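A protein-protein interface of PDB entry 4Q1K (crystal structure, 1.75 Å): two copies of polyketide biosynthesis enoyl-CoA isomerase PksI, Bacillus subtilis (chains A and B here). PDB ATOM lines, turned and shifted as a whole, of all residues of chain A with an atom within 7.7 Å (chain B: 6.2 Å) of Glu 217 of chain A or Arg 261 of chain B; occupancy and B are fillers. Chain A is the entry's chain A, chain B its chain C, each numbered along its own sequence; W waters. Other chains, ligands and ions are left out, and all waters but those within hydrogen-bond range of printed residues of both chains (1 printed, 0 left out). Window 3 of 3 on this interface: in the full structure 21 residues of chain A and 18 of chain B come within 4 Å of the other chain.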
ATOM      1  N   ALA A  33     -29.344  25.565  10.058  1.00  0.00           N
ATOM      2  CA  ALA A  33     -28.139  24.913  10.477  1.00  0.00           C
ATOM      3  C   ALA A  33     -27.293  24.621   9.266  1.00  0.00           C
ATOM      4  O   ALA A  33     -26.243  24.008   9.477  1.00  0.00           O
ATOM      5  CB  ALA A  33     -28.466  23.644  11.294  1.00  0.00           C
ATOM      6  N   ILE A  34     -27.629  25.111   8.046  1.00  0.00           N
ATOM      7  CA  ILE A  34     -26.722  24.775   6.876  1.00  0.00           C
ATOM      8  C   ILE A  34     -26.239  26.094   6.271  1.00  0.00           C
ATOM      9  O   ILE A  34     -27.031  27.015   6.076  1.00  0.00           O
ATOM     10  CB  ILE A  34     -27.519  24.012   5.812  1.00  0.00           C
ATOM     11  CG1 ILE A  34     -27.983  22.662   6.377  1.00  0.00           C
ATOM     12  CG2 ILE A  34     -26.704  23.811   4.485  1.00  0.00           C
ATOM     13  CD1 ILE A  34     -29.100  22.048   5.543  1.00  0.00           C
ATOM     14  N   LYS A  70     -24.441  23.280  11.317  1.00  0.00           N
ATOM     15  CA  LYS A  70     -24.076  21.910  11.488  1.00  0.00           C
ATOM     16  C   LYS A  70     -23.426  21.352  10.210  1.00  0.00           C
ATOM     17  O   LYS A  70     -22.899  20.286  10.246  1.00  0.00           O
ATOM     18  CB  LYS A  70     -25.292  21.048  11.795  1.00  0.00           C
ATOM     19  CG  LYS A  70     -25.888  21.264  13.206  1.00  0.00           C
ATOM     20  CD  LYS A  70     -27.121  20.395  13.324  1.00  0.00           C
ATOM     21  CE  LYS A  70     -27.761  20.456  14.684  1.00  0.00           C
ATOM     22  NZ  LYS A  70     -28.961  19.559  14.703  1.00  0.00           N
ATOM     23  N   GLU A 210     -29.582  18.234  -0.096  1.00  0.00           N
ATOM     24  CA  GLU A 210     -30.160  17.047   0.517  1.00  0.00           C
ATOM     25  C   GLU A 210     -29.290  16.377   1.550  1.00  0.00           C
ATOM     26  O   GLU A 210     -29.775  15.998   2.651  1.00  0.00           O
ATOM     27  CB  GLU A 210     -30.583  16.021  -0.536  1.00  0.00           C
ATOM     28  CG  GLU A 210     -31.784  16.497  -1.308  1.00  0.00           C
ATOM     29  CD  GLU A 210     -32.140  15.580  -2.480  1.00  0.00           C
ATOM     30  OE1 GLU A 210     -31.940  14.336  -2.366  1.00  0.00           O
ATOM     31  OE2 GLU A 210     -32.614  16.122  -3.515  1.00  0.00           O
ATOM     32  N   LEU A 211     -28.011  16.161   1.223  1.00  0.00           N
ATOM     33  CA  LEU A 211     -27.102  15.536   2.148  1.00  0.00           C
ATOM     34  C   LEU A 211     -26.862  16.416   3.352  1.00  0.00           C
ATOM     35  O   LEU A 211     -26.851  15.903   4.457  1.00  0.00           O
ATOM     36  CB  LEU A 211     -25.769  15.334   1.449  1.00  0.00           C
ATOM     37  CG  LEU A 211     -24.712  14.366   1.878  1.00  0.00           C
ATOM     38  CD1 LEU A 211     -25.315  13.167   2.592  1.00  0.00           C
ATOM     39  CD2 LEU A 211     -23.910  13.987   0.596  1.00  0.00           C
ATOM     40  N   ALA A 212     -26.682  17.728   3.171  1.00  0.00           N
ATOM     41  CA  ALA A 212     -26.547  18.659   4.311  1.00  0.00           C
ATOM     42  C   ALA A 212     -27.804  18.620   5.239  1.00  0.00           C
ATOM     43  O   ALA A 212     -27.661  18.668   6.495  1.00  0.00           O
ATOM     44  CB  ALA A 212     -26.265  20.103   3.794  1.00  0.00           C
ATOM     45  N   GLN A 213     -29.008  18.541   4.657  1.00  0.00           N
ATOM     46  CA  GLN A 213     -30.175  18.391   5.459  1.00  0.00           C
ATOM     47  C   GLN A 213     -30.110  17.146   6.325  1.00  0.00           C
ATOM     48  O   GLN A 213     -30.559  17.166   7.509  1.00  0.00           O
ATOM     49  CB  GLN A 213     -31.451  18.387   4.613  1.00  0.00           C
ATOM     50  CG  GLN A 213     -31.695  19.814   4.053  1.00  0.00           C
ATOM     51  CD  GLN A 213     -32.801  19.815   3.023  1.00  0.00           C
ATOM     52  OE1 GLN A 213     -32.858  18.977   2.147  1.00  0.00           O
ATOM     53  NE2 GLN A 213     -33.697  20.731   3.159  1.00  0.00           N
ATOM     54  N   GLU A 214     -29.661  16.039   5.755  1.00  0.00           N
ATOM     55  CA  GLU A 214     -29.609  14.811   6.553  1.00  0.00           C
ATOM     56  C   GLU A 214     -28.528  14.904   7.652  1.00  0.00           C
ATOM     57  O   GLU A 214     -28.729  14.356   8.745  1.00  0.00           O
ATOM     58  CB  GLU A 214     -29.385  13.571   5.654  1.00  0.00           C
ATOM     59  CG  GLU A 214     -30.520  13.436   4.619  1.00  0.00           C
ATOM     60  CD  GLU A 214     -30.224  12.427   3.517  1.00  0.00           C
ATOM     61  OE1 GLU A 214     -29.064  11.902   3.421  1.00  0.00           O
ATOM     62  OE2 GLU A 214     -31.157  12.216   2.711  1.00  0.00           O
ATOM     63  N   LEU A 215     -27.428  15.588   7.365  1.00  0.00           N
ATOM     64  CA  LEU A 215     -26.399  15.756   8.387  1.00  0.00           C
ATOM     65  C   LEU A 215     -26.996  16.609   9.506  1.00  0.00           C
ATOM     66  O   LEU A 215     -26.721  16.322  10.710  1.00  0.00           O
ATOM     67  CB  LEU A 215     -25.150  16.446   7.881  1.00  0.00           C
ATOM     68  CG  LEU A 215     -24.306  15.512   6.960  1.00  0.00           C
ATOM     69  CD1 LEU A 215     -23.269  16.272   6.119  1.00  0.00           C
ATOM     70  CD2 LEU A 215     -23.603  14.431   7.803  1.00  0.00           C
ATOM     71  N   ALA A 216     -27.761  17.629   9.151  1.00  0.00           N
ATOM     72  CA  ALA A 216     -28.256  18.574  10.186  1.00  0.00           C
ATOM     73  C   ALA A 216     -29.320  17.946  11.078  1.00  0.00           C
ATOM     74  O   ALA A 216     -29.785  18.586  12.038  1.00  0.00           O
ATOM     75  CB  ALA A 216     -28.756  19.889   9.522  1.00  0.00           C
ATOM     76  N   GLU A 217     -29.697  16.685  10.802  1.00  0.00           N
ATOM     77  CA  GLU A 217     -30.605  15.987  11.723  1.00  0.00           C
ATOM     78  C   GLU A 217     -29.862  15.510  12.963  1.00  0.00           C
ATOM     79  O   GLU A 217     -30.459  15.042  13.912  1.00  0.00           O
ATOM     80  CB  GLU A 217     -31.202  14.774  11.005  1.00  0.00           C
ATOM     81  CG  GLU A 217     -32.220  15.179   9.938  1.00  0.00           C
ATOM     82  CD  GLU A 217     -32.787  14.014   9.121  1.00  0.00           C
ATOM     83  OE1 GLU A 217     -32.381  12.847   9.342  1.00  0.00           O
ATOM     84  OE2 GLU A 217     -33.649  14.268   8.239  1.00  0.00           O
ATOM     85  N   LYS A 218     -28.542  15.538  12.955  1.00  0.00           N
ATOM     86  CA  LYS A 218     -27.706  14.968  14.021  1.00  0.00           C
ATOM     87  C   LYS A 218     -27.410  16.079  15.054  1.00  0.00           C
ATOM     88  O   LYS A 218     -27.352  17.295  14.660  1.00  0.00           O
ATOM     89  CB  LYS A 218     -26.359  14.486  13.470  1.00  0.00           C
ATOM     90  CG  LYS A 218     -26.393  13.067  12.861  1.00  0.00           C
ATOM     91  CD  LYS A 218     -27.373  12.928  11.684  1.00  0.00           C
ATOM     92  CE  LYS A 218     -26.952  11.803  10.695  1.00  0.00           C
ATOM     93  NZ  LYS A 218     -27.996  11.833   9.622  1.00  0.00           N
ATOM     94  N   PRO A 219     -27.217  15.700  16.342  1.00  0.00           N
ATOM     95  CA  PRO A 219     -26.743  16.715  17.329  1.00  0.00           C
ATOM     96  C   PRO A 219     -25.424  17.288  16.888  1.00  0.00           C
ATOM     97  O   PRO A 219     -24.526  16.504  16.453  1.00  0.00           O
ATOM     98  CB  PRO A 219     -26.477  15.875  18.617  1.00  0.00           C
ATOM     99  CG  PRO A 219     -27.320  14.649  18.453  1.00  0.00           C
ATOM    100  CD  PRO A 219     -27.217  14.348  16.946  1.00  0.00           C
ATOM    101  N   ARG A 220     -25.223  18.607  16.984  1.00  0.00           N
ATOM    102  CA  ARG A 220     -23.975  19.194  16.478  1.00  0.00           C
ATOM    103  C   ARG A 220     -22.789  18.596  17.238  1.00  0.00           C
ATOM    104  O   ARG A 220     -21.697  18.400  16.668  1.00  0.00           O
ATOM    105  CB  ARG A 220     -24.028  20.734  16.674  1.00  0.00           C
ATOM    106  CG  ARG A 220     -22.811  21.417  16.038  1.00  0.00           C
ATOM    107  CD  ARG A 220     -22.951  22.922  16.228  1.00  0.00           C
ATOM    108  NE  ARG A 220     -21.957  23.708  15.522  1.00  0.00           N
ATOM    109  CZ  ARG A 220     -20.718  23.929  15.931  1.00  0.00           C
ATOM    110  NH1 ARG A 220     -20.220  23.413  17.075  1.00  0.00           N
ATOM    111  NH2 ARG A 220     -19.946  24.673  15.174  1.00  0.00           N
ATOM    112  N   SER A 222     -22.328  15.753  18.309  1.00  0.00           N
ATOM    113  CA  SER A 222     -21.923  14.368  17.836  1.00  0.00           C
ATOM    114  C   SER A 222     -21.211  14.511  16.466  1.00  0.00           C
ATOM    115  O   SER A 222     -20.227  13.792  16.208  1.00  0.00           O
ATOM    116  CB  SER A 222     -23.175  13.500  17.627  1.00  0.00           C
ATOM    117  OG  SER A 222     -23.689  13.231  18.896  1.00  0.00           O
ATOM    118  N   LEU A 223     -21.724  15.414  15.607  1.00  0.00           N
ATOM    119  CA  LEU A 223     -21.025  15.693  14.285  1.00  0.00           C
ATOM    120  C   LEU A 223     -19.551  16.119  14.533  1.00  0.00           C
ATOM    121  O   LEU A 223     -18.615  15.642  13.886  1.00  0.00           O
ATOM    122  CB  LEU A 223     -21.717  16.778  13.432  1.00  0.00           C
ATOM    123  CG  LEU A 223     -23.132  16.364  13.003  1.00  0.00           C
ATOM    124  CD1 LEU A 223     -23.863  17.554  12.437  1.00  0.00           C
ATOM    125  CD2 LEU A 223     -23.009  15.311  11.823  1.00  0.00           C
ATOM    126  N   MET B 151     -25.294   7.156  14.201  1.00  0.00           N
ATOM    127  CA  MET B 151     -25.452   8.590  14.327  1.00  0.00           C
ATOM    128  C   MET B 151     -26.922   8.978  14.143  1.00  0.00           C
ATOM    129  O   MET B 151     -27.328  10.055  14.580  1.00  0.00           O
ATOM    130  CB  MET B 151     -24.566   9.372  13.366  1.00  0.00           C
ATOM    131  CG  MET B 151     -23.065   9.254  13.778  1.00  0.00           C
ATOM    132  SD  MET B 151     -22.658  10.552  15.029  1.00  0.00           S
ATOM    133  CE  MET B 151     -22.533  12.042  13.997  1.00  0.00           C
ATOM    134  N   LYS B 152     -27.716   8.135  13.507  1.00  0.00           N
ATOM    135  CA  LYS B 152     -29.173   8.471  13.420  1.00  0.00           C
ATOM    136  C   LYS B 152     -29.791   8.662  14.833  1.00  0.00           C
ATOM    137  O   LYS B 152     -30.762   9.430  15.005  1.00  0.00           O
ATOM    138  CB  LYS B 152     -29.902   7.325  12.658  1.00  0.00           C
ATOM    139  CG  LYS B 152     -31.410   7.377  12.779  1.00  0.00           C
ATOM    140  CD  LYS B 152     -32.044   6.187  12.023  1.00  0.00           C
ATOM    141  CE  LYS B 152     -32.284   4.975  12.913  1.00  0.00           C
ATOM    142  NZ  LYS B 152     -33.255   3.987  12.329  1.00  0.00           N
ATOM    143  N   TYR B 153     -29.245   7.939  15.820  1.00  0.00           N
ATOM    144  CA  TYR B 153     -29.758   7.970  17.193  1.00  0.00           C
ATOM    145  C   TYR B 153     -29.068   9.018  17.983  1.00  0.00           C
ATOM    146  O   TYR B 153     -29.316   9.116  19.203  1.00  0.00           O
ATOM    147  CB  TYR B 153     -29.503   6.606  17.898  1.00  0.00           C
ATOM    148  CG  TYR B 153     -30.309   5.491  17.200  1.00  0.00           C
ATOM    149  CD1 TYR B 153     -31.738   5.552  17.128  1.00  0.00           C
ATOM    150  CD2 TYR B 153     -29.658   4.447  16.553  1.00  0.00           C
ATOM    151  CE1 TYR B 153     -32.460   4.563  16.463  1.00  0.00           C
ATOM    152  CE2 TYR B 153     -30.363   3.439  15.905  1.00  0.00           C
ATOM    153  CZ  TYR B 153     -31.747   3.510  15.839  1.00  0.00           C
ATOM    154  OH  TYR B 153     -32.406   2.511  15.119  1.00  0.00           O
ATOM    155  N   GLY B 154     -28.122   9.719  17.360  1.00  0.00           N
ATOM    156  CA  GLY B 154     -27.490  10.855  18.049  1.00  0.00           C
ATOM    157  C   GLY B 154     -26.164  10.514  18.683  1.00  0.00           C
ATOM    158  O   GLY B 154     -25.489  11.421  19.219  1.00  0.00           O
ATOM    159  N   GLU B 256     -30.216  13.202  26.964  1.00  0.00           N
ATOM    160  CA  GLU B 256     -31.627  12.854  26.841  1.00  0.00           C
ATOM    161  C   GLU B 256     -32.083  12.727  25.376  1.00  0.00           C
ATOM    162  O   GLU B 256     -32.910  11.859  25.068  1.00  0.00           O
ATOM    163  CB  GLU B 256     -32.532  13.845  27.593  1.00  0.00           C
ATOM    164  CG  GLU B 256     -34.010  13.426  27.747  1.00  0.00           C
ATOM    165  CD  GLU B 256     -34.253  12.187  28.632  1.00  0.00           C
ATOM    166  OE1 GLU B 256     -33.410  11.793  29.501  1.00  0.00           O
ATOM    167  OE2 GLU B 256     -35.324  11.580  28.430  1.00  0.00           O
ATOM    168  N   GLU B 257     -31.563  13.563  24.487  1.00  0.00           N
ATOM    169  CA  GLU B 257     -32.092  13.477  23.162  1.00  0.00           C
ATOM    170  C   GLU B 257     -31.714  12.134  22.535  1.00  0.00           C
ATOM    171  O   GLU B 257     -32.455  11.658  21.673  1.00  0.00           O
ATOM    172  CB  GLU B 257     -31.750  14.682  22.269  1.00  0.00           C
ATOM    173  CG  GLU B 257     -30.320  14.784  21.791  1.00  0.00           C
ATOM    174  CD  GLU B 257     -30.132  15.961  20.818  1.00  0.00           C
ATOM    175  OE1 GLU B 257     -29.240  16.844  21.052  1.00  0.00           O
ATOM    176  OE2 GLU B 257     -30.886  16.014  19.810  1.00  0.00           O
ATOM    177  N   VAL B 258     -30.577  11.522  22.928  1.00  0.00           N
ATOM    178  CA  VAL B 258     -30.261  10.149  22.441  1.00  0.00           C
ATOM    179  C   VAL B 258     -31.351   9.162  22.870  1.00  0.00           C
ATOM    180  O   VAL B 258     -31.804   8.307  22.061  1.00  0.00           O
ATOM    181  CB  VAL B 258     -28.867   9.675  22.939  1.00  0.00           C
ATOM    182  CG1 VAL B 258     -28.656   8.189  22.682  1.00  0.00           C
ATOM    183  CG2 VAL B 258     -27.794  10.594  22.361  1.00  0.00           C
ATOM    184  N   LYS B 259     -31.835   9.299  24.114  1.00  0.00           N
ATOM    185  CA  LYS B 259     -32.870   8.375  24.624  1.00  0.00           C
ATOM    186  C   LYS B 259     -34.127   8.631  23.791  1.00  0.00           C
ATOM    187  O   LYS B 259     -34.791   7.667  23.385  1.00  0.00           O
ATOM    188  CB  LYS B 259     -33.112   8.608  26.114  1.00  0.00           C
ATOM    189  CG  LYS B 259     -34.234   7.766  26.713  1.00  0.00           C
ATOM    190  CD  LYS B 259     -34.292   7.980  28.236  1.00  0.00           C
ATOM    191  CE  LYS B 259     -35.712   8.270  28.681  1.00  0.00           C
ATOM    192  NZ  LYS B 259     -35.905   7.711  30.043  1.00  0.00           N
ATOM    193  N   SER B 260     -34.445   9.899  23.488  1.00  0.00           N
ATOM    194  CA  SER B 260     -35.675  10.172  22.660  1.00  0.00           C
ATOM    195  C   SER B 260     -35.586   9.556  21.271  1.00  0.00           C
ATOM    196  O   SER B 260     -36.562   8.972  20.804  1.00  0.00           O
ATOM    197  CB  SER B 260     -35.984  11.650  22.458  1.00  0.00           C
ATOM    198  OG  SER B 260     -36.150  12.199  23.726  1.00  0.00           O
ATOM    199  N   ARG B 261     -34.419   9.704  20.630  1.00  0.00           N
ATOM    200  CA  ARG B 261     -34.213   9.158  19.261  1.00  0.00           C
ATOM    201  C   ARG B 261     -34.260   7.650  19.192  1.00  0.00           C
ATOM    202  O   ARG B 261     -34.837   7.111  18.251  1.00  0.00           O
ATOM    203  CB  ARG B 261     -32.938   9.646  18.626  1.00  0.00           C
ATOM    204  CG  ARG B 261     -32.906  11.125  18.502  1.00  0.00           C
ATOM    205  CD  ARG B 261     -31.562  11.476  18.047  1.00  0.00           C
ATOM    206  NE  ARG B 261     -31.459  12.889  17.811  1.00  0.00           N
ATOM    207  CZ  ARG B 261     -30.981  13.422  16.700  1.00  0.00           C
ATOM    208  NH1 ARG B 261     -30.516  12.632  15.700  1.00  0.00           N
ATOM    209  NH2 ARG B 261     -30.919  14.754  16.627  1.00  0.00           N
ATOM    210  N   ILE B 262     -33.696   6.981  20.175  1.00  0.00           N
ATOM    211  CA  ILE B 262     -33.743   5.533  20.227  1.00  0.00           C
ATOM    212  C   ILE B 262     -35.226   5.118  20.386  1.00  0.00           C
ATOM    213  O   ILE B 262     -35.710   4.195  19.689  1.00  0.00           O
ATOM    214  CB  ILE B 262     -32.920   4.962  21.377  1.00  0.00           C
ATOM    215  CG1 ILE B 262     -31.405   5.133  21.169  1.00  0.00           C
ATOM    216  CG2 ILE B 262     -33.276   3.485  21.607  1.00  0.00           C
ATOM    217  CD1 ILE B 262     -30.599   4.801  22.417  1.00  0.00           C
ATOM    218  N   LYS B 263     -35.950   5.812  21.297  1.00  0.00           N
ATOM    219  CA  LYS B 263     -37.394   5.513  21.518  1.00  0.00           C
ATOM    220  C   LYS B 263     -38.224   5.786  20.287  1.00  0.00           C
ATOM    221  O   LYS B 263     -39.083   4.967  19.919  1.00  0.00           O
ATOM    222  CB  LYS B 263     -37.993   6.208  22.773  1.00  0.00           C
ATOM    223  CG  LYS B 263     -37.496   5.563  24.058  1.00  0.00           C
ATOM    224  CD  LYS B 263     -38.581   5.492  25.123  1.00  0.00           C
ATOM    225  CE  LYS B 263     -38.020   5.563  26.544  1.00  0.00           C
ATOM    226  NZ  LYS B 263     -38.187   6.925  27.165  1.00  0.00           N
ATOM    227  N   GLY B 264     -37.965   6.900  19.623  1.00  0.00           N
ATOM    228  CA  GLY B 264     -38.734   7.266  18.463  1.00  0.00           C
ATOM    229  C   GLY B 264     -38.289   6.839  17.059  1.00  0.00           C
ATOM    230  O   GLY B 264     -39.114   6.901  16.131  1.00  0.00           O
ATOM    231  N   LEU B 265     -37.030   6.401  16.842  1.00  0.00           N
ATOM    232  CA  LEU B 265     -36.606   6.181  15.450  1.00  0.00           C
ATOM    233  C   LEU B 265     -36.253   4.716  15.221  1.00  0.00           C
ATOM    234  O   LEU B 265     -36.009   4.331  14.077  1.00  0.00           O
ATOM    235  CB  LEU B 265     -35.411   7.097  15.062  1.00  0.00           C
ATOM    236  CG  LEU B 265     -35.573   8.595  15.164  1.00  0.00           C
ATOM    237  CD1 LEU B 265     -34.290   9.363  14.878  1.00  0.00           C
ATOM    238  CD2 LEU B 265     -36.691   9.109  14.237  1.00  0.00           C
ATOM    239  N   TYR B 266     -36.203   3.915  16.294  1.00  0.00           N
ATOM    240  CA  TYR B 266     -35.759   2.521  16.174  1.00  0.00           C
ATOM    241  C   TYR B 266     -36.669   1.773  15.203  1.00  0.00           C
ATOM    242  O   TYR B 266     -37.868   1.912  15.297  1.00  0.00           O
ATOM    243  CB  TYR B 266     -35.758   1.820  17.537  1.00  0.00           C
ATOM    244  CG  TYR B 266     -35.027   0.499  17.492  1.00  0.00           C
ATOM    245  CD1 TYR B 266     -33.620   0.431  17.752  1.00  0.00           C
ATOM    246  CD2 TYR B 266     -35.717  -0.704  17.181  1.00  0.00           C
ATOM    247  CE1 TYR B 266     -32.961  -0.746  17.687  1.00  0.00           C
ATOM    248  CE2 TYR B 266     -35.042  -1.915  17.099  1.00  0.00           C
ATOM    249  CZ  TYR B 266     -33.680  -1.911  17.337  1.00  0.00           C
ATOM    250  OH  TYR B 266     -33.008  -3.039  17.309  1.00  0.00           O
HETATM  251  O   HOH W   1     -25.693  13.094  21.492  1.00  0.00           O
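The side-chain hydroxyl of Ser 222 of chain A sits at hydrogen-bond distance from the backbone carbonyl oxygen of Gly 154 of chain B, at 2.6 Å. O of Glu 217 of chain A lies within hydrogen-bond range of NH2 of Arg 261 of chain B (2.8 Å).
No position is printed for both chains. Of the 8 pairs that touch across the chains among the printed residues, none has its exchanged pair printed and touching as well.
Water W1 bridges O of Gly 154 of chain B (2.8 Å) and OG of Ser 222 of chain A (3.3 Å).
Among the printed residues, pairs that only touch across the chains: Lys 218 of chain A with Met 151 of chain B, Pro 219 of chain A with Gly 154 of chain B, Pro 219 of chain A with Glu 257 of chain B, Pro 219 of chain A with Arg 261 of chain B, Ser 222 of chain A with Met 151 of chain B and Leu 223 of chain A with Met 151 of chain B.
Printed residues of chain B within 4 Å of Glu 217 of chain A: Arg 261. Of chain A, only Glu 217 and Pro 219 come within 4 Å of Arg 261 of chain B. Of the printed residues of chain A, Glu 257 of chain B touches Pro 219. Of the printed residues of chain B, Pro 219 of chain A touches Gly 154, Glu 257 and Arg 261. Ile 262 of chain B touches none of the printed residues of chain A. The nearest residue of chain A that does not touch Arg 261 of chain B is Lys 218 of chain A (4.02 Å).
The backbone carbonyl oxygen of Glu 214 of chain A sits at hydrogen-bond distance from the side-chain amino group of Lys 218 of chain A. NZ of Lys 70 of chain A lies within hydrogen-bond range of O of Lys 218 of chain A. NH2 of Arg 261 of chain B is in salt-bridge range of OE2 of Glu 257 of chain B, 3.4 Å away. NH1 of Arg 261 of chain B lies within hydrogen-bond range of O of Lys 152 of chain B (3.3 Å).
Of the 16 printed residues of chain A, 5 touch a printed residue of chain B. Printed residues of chain B that touch a printed residue of chain A: Met 151, Gly 154, Glu 257 and Arg 261. Among the printed residues, 8 pairs touch across the chains.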
